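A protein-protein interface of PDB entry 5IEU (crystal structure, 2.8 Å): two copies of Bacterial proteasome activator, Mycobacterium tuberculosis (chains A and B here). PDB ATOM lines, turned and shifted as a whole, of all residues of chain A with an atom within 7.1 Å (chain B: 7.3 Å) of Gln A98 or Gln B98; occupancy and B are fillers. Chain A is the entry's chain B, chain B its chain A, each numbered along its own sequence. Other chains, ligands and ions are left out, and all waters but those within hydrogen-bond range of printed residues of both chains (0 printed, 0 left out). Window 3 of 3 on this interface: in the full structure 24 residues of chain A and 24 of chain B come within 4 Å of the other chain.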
ATOM      1  N   VAL A   5     -11.648  12.678  25.487  1.00  0.00           N
ATOM      2  CA  VAL A   5     -12.989  12.560  26.172  1.00  0.00           C
ATOM      3  C   VAL A   5     -14.192  12.226  25.228  1.00  0.00           C
ATOM      4  O   VAL A   5     -14.616  13.038  24.367  1.00  0.00           O
ATOM      5  CB  VAL A   5     -13.298  13.792  27.069  1.00  0.00           C
ATOM      6  CG1 VAL A   5     -12.261  13.910  28.192  1.00  0.00           C
ATOM      7  CG2 VAL A   5     -13.388  15.077  26.244  1.00  0.00           C
ATOM      8  N   GLN A  92     -14.506   5.839  17.069  1.00  0.00           N
ATOM      9  CA  GLN A  92     -13.992   4.608  17.618  1.00  0.00           C
ATOM     10  C   GLN A  92     -12.661   4.145  16.973  1.00  0.00           C
ATOM     11  O   GLN A  92     -11.694   3.860  17.657  1.00  0.00           O
ATOM     12  CB  GLN A  92     -15.036   3.525  17.483  1.00  0.00           C
ATOM     13  CG  GLN A  92     -14.660   2.309  18.280  1.00  0.00           C
ATOM     14  CD  GLN A  92     -15.860   1.488  18.707  1.00  0.00           C
ATOM     15  OE1 GLN A  92     -16.796   1.298  17.942  1.00  0.00           O
ATOM     16  NE2 GLN A  92     -15.818   0.964  19.927  1.00  0.00           N
ATOM     17  N   THR A  93     -12.592   4.098  15.654  1.00  0.00           N
ATOM     18  CA  THR A  93     -11.373   3.583  15.046  1.00  0.00           C
ATOM     19  C   THR A  93     -10.208   4.526  15.237  1.00  0.00           C
ATOM     20  O   THR A  93      -9.081   4.081  15.433  1.00  0.00           O
ATOM     21  CB  THR A  93     -11.498   3.247  13.557  1.00  0.00           C
ATOM     22  OG1 THR A  93     -11.486   4.450  12.802  1.00  0.00           O
ATOM     23  CG2 THR A  93     -12.759   2.366  13.299  1.00  0.00           C
ATOM     24  N   ALA A  94     -10.482   5.827  15.204  1.00  0.00           N
ATOM     25  CA  ALA A  94      -9.460   6.836  15.457  1.00  0.00           C
ATOM     26  C   ALA A  94      -8.876   6.665  16.850  1.00  0.00           C
ATOM     27  O   ALA A  94      -7.663   6.819  17.069  1.00  0.00           O
ATOM     28  CB  ALA A  94     -10.044   8.237  15.281  1.00  0.00           C
ATOM     29  N   LEU A  95      -9.747   6.358  17.801  1.00  0.00           N
ATOM     30  CA  LEU A  95      -9.355   6.149  19.220  1.00  0.00           C
ATOM     31  C   LEU A  95      -8.429   4.935  19.361  1.00  0.00           C
ATOM     32  O   LEU A  95      -7.515   4.881  20.184  1.00  0.00           O
ATOM     33  CB  LEU A  95     -10.615   5.948  20.073  1.00  0.00           C
ATOM     34  CG  LEU A  95     -11.026   7.151  20.909  1.00  0.00           C
ATOM     35  CD1 LEU A  95     -12.426   7.023  21.461  1.00  0.00           C
ATOM     36  CD2 LEU A  95     -10.071   7.292  22.083  1.00  0.00           C
ATOM     37  N   PHE A  96      -8.691   3.957  18.525  1.00  0.00           N
ATOM     38  CA  PHE A  96      -7.876   2.773  18.468  1.00  0.00           C
ATOM     39  C   PHE A  96      -6.530   2.990  17.838  1.00  0.00           C
ATOM     40  O   PHE A  96      -5.520   2.503  18.314  1.00  0.00           O
ATOM     41  CB  PHE A  96      -8.588   1.714  17.653  1.00  0.00           C
ATOM     42  CG  PHE A  96      -8.116   0.325  17.953  1.00  0.00           C
ATOM     43  CD1 PHE A  96      -8.601  -0.357  19.064  1.00  0.00           C
ATOM     44  CD2 PHE A  96      -7.187  -0.291  17.134  1.00  0.00           C
ATOM     45  CE1 PHE A  96      -8.165  -1.628  19.342  1.00  0.00           C
ATOM     46  CE2 PHE A  96      -6.747  -1.562  17.413  1.00  0.00           C
ATOM     47  CZ  PHE A  96      -7.231  -2.229  18.515  1.00  0.00           C
ATOM     48  N   ALA A  97      -6.535   3.666  16.709  1.00  0.00           N
ATOM     49  CA  ALA A  97      -5.312   4.169  16.125  1.00  0.00           C
ATOM     50  C   ALA A  97      -4.461   4.841  17.180  1.00  0.00           C
ATOM     51  O   ALA A  97      -3.266   4.677  17.247  1.00  0.00           O
ATOM     52  CB  ALA A  97      -5.657   5.177  15.059  1.00  0.00           C
ATOM     53  N   GLN A  98      -5.079   5.625  18.026  1.00  0.00           N
ATOM     54  CA  GLN A  98      -4.287   6.380  18.988  1.00  0.00           C
ATOM     55  C   GLN A  98      -3.530   5.441  19.979  1.00  0.00           C
ATOM     56  O   GLN A  98      -2.323   5.540  20.197  1.00  0.00           O
ATOM     57  CB  GLN A  98      -5.225   7.352  19.720  1.00  0.00           C
ATOM     58  CG  GLN A  98      -4.539   8.524  20.342  1.00  0.00           C
ATOM     59  CD  GLN A  98      -5.316   9.083  21.514  1.00  0.00           C
ATOM     60  OE1 GLN A  98      -6.529   9.306  21.420  1.00  0.00           O
ATOM     61  NE2 GLN A  98      -4.610   9.355  22.623  1.00  0.00           N
ATOM     62  N   GLN A  99      -4.283   4.555  20.595  1.00  0.00           N
ATOM     63  CA  GLN A  99      -3.731   3.562  21.485  1.00  0.00           C
ATOM     64  C   GLN A  99      -2.646   2.709  20.790  1.00  0.00           C
ATOM     65  O   GLN A  99      -1.624   2.335  21.381  1.00  0.00           O
ATOM     66  CB  GLN A  99      -4.862   2.655  21.954  1.00  0.00           C
ATOM     67  CG  GLN A  99      -4.351   1.498  22.744  1.00  0.00           C
ATOM     68  CD  GLN A  99      -5.386   0.439  22.934  1.00  0.00           C
ATOM     69  OE1 GLN A  99      -6.585   0.684  22.719  1.00  0.00           O
ATOM     70  NE2 GLN A  99      -4.932  -0.764  23.366  1.00  0.00           N
ATOM     71  N   MET A 100      -2.893   2.385  19.531  1.00  0.00           N
ATOM     72  CA  MET A 100      -1.996   1.527  18.766  1.00  0.00           C
ATOM     73  C   MET A 100      -0.743   2.212  18.333  1.00  0.00           C
ATOM     74  O   MET A 100       0.297   1.591  18.246  1.00  0.00           O
ATOM     75  CB  MET A 100      -2.701   1.016  17.527  1.00  0.00           C
ATOM     76  CG  MET A 100      -3.795   0.006  17.866  1.00  0.00           C
ATOM     77  SD  MET A 100      -3.215  -1.451  18.800  1.00  0.00           S
ATOM     78  CE  MET A 100      -3.659  -1.105  20.503  1.00  0.00           C
ATOM     79  N   ALA A 101      -0.843   3.488  18.040  1.00  0.00           N
ATOM     80  CA  ALA A 101       0.339   4.270  17.726  1.00  0.00           C
ATOM     81  C   ALA A 101       1.239   4.465  18.964  1.00  0.00           C
ATOM     82  O   ALA A 101       2.456   4.288  18.869  1.00  0.00           O
ATOM     83  CB  ALA A 101      -0.064   5.614  17.138  1.00  0.00           C
ATOM     84  N   ALA A 102       0.654   4.820  20.114  1.00  0.00           N
ATOM     85  CA  ALA A 102       1.446   4.997  21.319  1.00  0.00           C
ATOM     86  C   ALA A 102       2.243   3.700  21.658  1.00  0.00           C
ATOM     87  O   ALA A 102       3.401   3.801  22.067  1.00  0.00           O
ATOM     88  CB  ALA A 102       0.567   5.451  22.487  1.00  0.00           C
ATOM     89  N   ARG A 103       1.614   2.515  21.473  1.00  0.00           N
ATOM     90  CA  ARG A 103       2.223   1.183  21.667  1.00  0.00           C
ATOM     91  C   ARG A 103       3.413   0.929  20.721  1.00  0.00           C
ATOM     92  O   ARG A 103       4.474   0.464  21.119  1.00  0.00           O
ATOM     93  CB  ARG A 103       1.172   0.080  21.446  1.00  0.00           C
ATOM     94  CG  ARG A 103       1.579  -1.284  22.004  1.00  0.00           C
ATOM     95  CD  ARG A 103       0.778  -2.457  21.429  1.00  0.00           C
ATOM     96  NE  ARG A 103      -0.061  -3.176  22.417  1.00  0.00           N
ATOM     97  CZ  ARG A 103      -0.722  -4.328  22.184  1.00  0.00           C
ATOM     98  NH1 ARG A 103      -0.673  -4.942  20.988  1.00  0.00           N
ATOM     99  NH2 ARG A 103      -1.455  -4.884  23.154  1.00  0.00           N
ATOM    100  N   ALA A 104       3.210   1.198  19.448  1.00  0.00           N
ATOM    101  CA  ALA A 104       4.288   1.078  18.450  1.00  0.00           C
ATOM    102  C   ALA A 104       5.485   1.950  18.808  1.00  0.00           C
ATOM    103  O   ALA A 104       6.621   1.473  18.908  1.00  0.00           O
ATOM    104  CB  ALA A 104       3.775   1.478  17.074  1.00  0.00           C
ATOM    105  N   VAL B   5      -4.550   6.702   9.838  1.00  0.00           N
ATOM    106  CA  VAL B   5      -5.783   7.472   9.924  1.00  0.00           C
ATOM    107  C   VAL B   5      -5.975   8.469   8.765  1.00  0.00           C
ATOM    108  O   VAL B   5      -7.106   8.793   8.356  1.00  0.00           O
ATOM    109  CB  VAL B   5      -5.844   8.196  11.294  1.00  0.00           C
ATOM    110  CG1 VAL B   5      -6.531   9.544  11.170  1.00  0.00           C
ATOM    111  CG2 VAL B   5      -6.555   7.317  12.327  1.00  0.00           C
ATOM    112  N   GLN B  92     -12.223  13.233  12.800  1.00  0.00           N
ATOM    113  CA  GLN B  92     -11.754  14.590  12.945  1.00  0.00           C
ATOM    114  C   GLN B  92     -11.891  15.092  14.365  1.00  0.00           C
ATOM    115  O   GLN B  92     -10.975  15.699  14.918  1.00  0.00           O
ATOM    116  CB  GLN B  92     -12.531  15.507  12.045  1.00  0.00           C
ATOM    117  CG  GLN B  92     -11.758  15.888  10.793  1.00  0.00           C
ATOM    118  CD  GLN B  92     -12.158  17.260  10.291  1.00  0.00           C
ATOM    119  OE1 GLN B  92     -12.762  18.072  11.019  1.00  0.00           O
ATOM    120  NE2 GLN B  92     -11.832  17.528   9.050  1.00  0.00           N
ATOM    121  N   THR B  93     -13.031  14.849  14.976  1.00  0.00           N
ATOM    122  CA  THR B  93     -13.207  15.342  16.332  1.00  0.00           C
ATOM    123  C   THR B  93     -12.401  14.523  17.356  1.00  0.00           C
ATOM    124  O   THR B  93     -12.031  15.072  18.378  1.00  0.00           O
ATOM    125  CB  THR B  93     -14.702  15.463  16.740  1.00  0.00           C
ATOM    126  OG1 THR B  93     -15.279  14.154  16.964  1.00  0.00           O
ATOM    127  CG2 THR B  93     -15.502  16.268  15.638  1.00  0.00           C
ATOM    128  N   ALA B  94     -12.127  13.232  17.088  1.00  0.00           N
ATOM    129  CA  ALA B  94     -11.257  12.402  18.001  1.00  0.00           C
ATOM    130  C   ALA B  94      -9.847  12.941  18.002  1.00  0.00           C
ATOM    131  O   ALA B  94      -9.230  13.080  19.081  1.00  0.00           O
ATOM    132  CB  ALA B  94     -11.248  10.916  17.638  1.00  0.00           C
ATOM    133  N   LEU B  95      -9.371  13.256  16.795  1.00  0.00           N
ATOM    134  CA  LEU B  95      -8.112  14.004  16.574  1.00  0.00           C
ATOM    135  C   LEU B  95      -7.986  15.367  17.263  1.00  0.00           C
ATOM    136  O   LEU B  95      -6.948  15.664  17.845  1.00  0.00           O
ATOM    137  CB  LEU B  95      -7.877  14.245  15.072  1.00  0.00           C
ATOM    138  CG  LEU B  95      -7.337  13.049  14.277  1.00  0.00           C
ATOM    139  CD1 LEU B  95      -7.209  13.433  12.818  1.00  0.00           C
ATOM    140  CD2 LEU B  95      -5.984  12.579  14.797  1.00  0.00           C
ATOM    141  N   PHE B  96      -9.011  16.214  17.146  1.00  0.00           N
ATOM    142  CA  PHE B  96      -8.984  17.529  17.804  1.00  0.00           C
ATOM    143  C   PHE B  96      -9.008  17.453  19.317  1.00  0.00           C
ATOM    144  O   PHE B  96      -8.412  18.275  20.000  1.00  0.00           O
ATOM    145  CB  PHE B  96     -10.156  18.396  17.375  1.00  0.00           C
ATOM    146  CG  PHE B  96     -10.010  19.833  17.820  1.00  0.00           C
ATOM    147  CD1 PHE B  96      -9.263  20.748  17.061  1.00  0.00           C
ATOM    148  CD2 PHE B  96     -10.570  20.267  19.034  1.00  0.00           C
ATOM    149  CE1 PHE B  96      -9.115  22.071  17.485  1.00  0.00           C
ATOM    150  CE2 PHE B  96     -10.423  21.587  19.457  1.00  0.00           C
ATOM    151  CZ  PHE B  96      -9.692  22.490  18.685  1.00  0.00           C
ATOM    152  N   ALA B  97      -9.731  16.477  19.832  1.00  0.00           N
ATOM    153  CA  ALA B  97      -9.813  16.246  21.269  1.00  0.00           C
ATOM    154  C   ALA B  97      -8.456  15.771  21.802  1.00  0.00           C
ATOM    155  O   ALA B  97      -8.009  16.221  22.889  1.00  0.00           O
ATOM    156  CB  ALA B  97     -10.889  15.196  21.562  1.00  0.00           C
ATOM    157  N   GLN B  98      -7.834  14.842  21.051  1.00  0.00           N
ATOM    158  CA  GLN B  98      -6.507  14.355  21.354  1.00  0.00           C
ATOM    159  C   GLN B  98      -5.473  15.491  21.431  1.00  0.00           C
ATOM    160  O   GLN B  98      -4.569  15.516  22.296  1.00  0.00           O
ATOM    161  CB  GLN B  98      -6.077  13.364  20.272  1.00  0.00           C
ATOM    162  CG  GLN B  98      -4.820  12.586  20.674  1.00  0.00           C
ATOM    163  CD  GLN B  98      -4.071  12.004  19.498  1.00  0.00           C
ATOM    164  OE1 GLN B  98      -4.641  11.778  18.426  1.00  0.00           O
ATOM    165  NE2 GLN B  98      -2.773  11.762  19.695  1.00  0.00           N
ATOM    166  N   GLN B  99      -5.611  16.416  20.491  1.00  0.00           N
ATOM    167  CA  GLN B  99      -4.758  17.586  20.394  1.00  0.00           C
ATOM    168  C   GLN B  99      -5.017  18.604  21.513  1.00  0.00           C
ATOM    169  O   GLN B  99      -4.103  19.241  22.024  1.00  0.00           O
ATOM    170  CB  GLN B  99      -4.997  18.278  19.057  1.00  0.00           C
ATOM    171  CG  GLN B  99      -4.744  19.774  19.124  1.00  0.00           C
ATOM    172  CD  GLN B  99      -4.726  20.397  17.763  1.00  0.00           C
ATOM    173  OE1 GLN B  99      -5.299  19.861  16.799  1.00  0.00           O
ATOM    174  NE2 GLN B  99      -4.027  21.522  17.653  1.00  0.00           N
ATOM    175  N   MET B 100      -6.279  18.805  21.853  1.00  0.00           N
ATOM    176  CA  MET B 100      -6.624  19.704  22.960  1.00  0.00           C
ATOM    177  C   MET B 100      -6.206  19.151  24.347  1.00  0.00           C
ATOM    178  O   MET B 100      -5.687  19.902  25.187  1.00  0.00           O
ATOM    179  CB  MET B 100      -8.128  20.075  22.918  1.00  0.00           C
ATOM    180  CG  MET B 100      -8.494  21.106  21.831  1.00  0.00           C
ATOM    181  SD  MET B 100      -7.489  22.636  21.767  1.00  0.00           S
ATOM    182  CE  MET B 100      -6.412  22.403  20.348  1.00  0.00           C
ATOM    183  N   ALA B 101      -6.396  17.851  24.582  1.00  0.00           N
ATOM    184  CA  ALA B 101      -5.993  17.212  25.863  1.00  0.00           C
ATOM    185  C   ALA B 101      -4.493  17.306  26.174  1.00  0.00           C
ATOM    186  O   ALA B 101      -4.105  17.533  27.332  1.00  0.00           O
ATOM    187  CB  ALA B 101      -6.401  15.751  25.879  1.00  0.00           C
ATOM    188  N   ALA B 102      -3.668  17.084  25.144  1.00  0.00           N
ATOM    189  CA  ALA B 102      -2.205  17.350  25.203  1.00  0.00           C
ATOM    190  C   ALA B 102      -1.884  18.819  25.437  1.00  0.00           C
ATOM    191  O   ALA B 102      -0.934  19.094  26.153  1.00  0.00           O
ATOM    192  CB  ALA B 102      -1.483  16.851  23.951  1.00  0.00           C
ATOM    193  N   ARG B 103      -2.667  19.742  24.854  1.00  0.00           N
ATOM    194  CA  ARG B 103      -2.469  21.176  25.047  1.00  0.00           C
ATOM    195  C   ARG B 103      -2.679  21.514  26.490  1.00  0.00           C
ATOM    196  O   ARG B 103      -1.850  22.125  27.124  1.00  0.00           O
ATOM    197  CB  ARG B 103      -3.430  21.986  24.197  1.00  0.00           C
ATOM    198  CG  ARG B 103      -3.138  23.475  24.218  1.00  0.00           C
ATOM    199  CD  ARG B 103      -4.005  24.275  23.252  1.00  0.00           C
ATOM    200  NE  ARG B 103      -3.696  25.721  23.282  1.00  0.00           N
ATOM    201  CZ  ARG B 103      -4.366  26.649  22.595  1.00  0.00           C
ATOM    202  NH1 ARG B 103      -5.375  26.267  21.805  1.00  0.00           N
ATOM    203  NH2 ARG B 103      -4.041  27.951  22.690  1.00  0.00           N
ATOM    204  N   GLN B 105      -2.750  19.652  29.214  1.00  0.00           N
ATOM    205  CA  GLN B 105      -1.789  18.997  30.076  1.00  0.00           C
ATOM    206  C   GLN B 105      -0.482  19.730  30.050  1.00  0.00           C
ATOM    207  O   GLN B 105       0.196  19.817  31.046  1.00  0.00           O
ATOM    208  CB  GLN B 105      -1.600  17.553  29.645  1.00  0.00           C
ATOM    209  CG  GLN B 105      -2.546  16.631  30.394  1.00  0.00           C
ATOM    210  CD  GLN B 105      -2.459  15.175  29.945  1.00  0.00           C
ATOM    211  OE1 GLN B 105      -2.520  14.888  28.744  1.00  0.00           O
ATOM    212  NE2 GLN B 105      -2.362  14.237  30.913  1.00  0.00           N
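Of chain B, only Gln B98 comes within 4 Å of Gln A98. Gln B98 touches one residue of chain A. Of the printed residues of chain A, Val B5 touches Ala A97 (3.6 Å). Printed residues of chain B within 4 Å of Ala A94: Ala B94 (3.8 Å). Leu B95 touches none of the printed residues of chain A. Met B100 touches none of the printed residues of chain A. The nearest residue of chain A that does not touch Gln B98 is Ala A94 (6.0 Å).
Hydrophobic or aromatic side chains of chain B within 4 Å of the printed part of chain A: Val B5 and Ala B94. Of the 14 printed residues of chain A, 3 touch a printed residue of chain B.
Ala B94 touches Ala A94. Ala A97 touches Val B5 (CB to CG2, 3.6 Å). Gln A98 touches Gln B98 (CG to CD, 3.6 Å).
Ala B94 touches its own counterpart, Ala A94. Ala A97 touches Val B5, but with the chains exchanged Val A5 does not touch Ala B97 (4.7 Å). Gln B98 touches its own counterpart, Gln A98. Positions printed for both chains: 5, 92, 93, 94, 95, 96, 97, 98, 99, 100, 101, 102 and 103. Of the 3 pairs that touch across the chains among the printed residues, 2 have their exchanged pair printed and touching as well.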
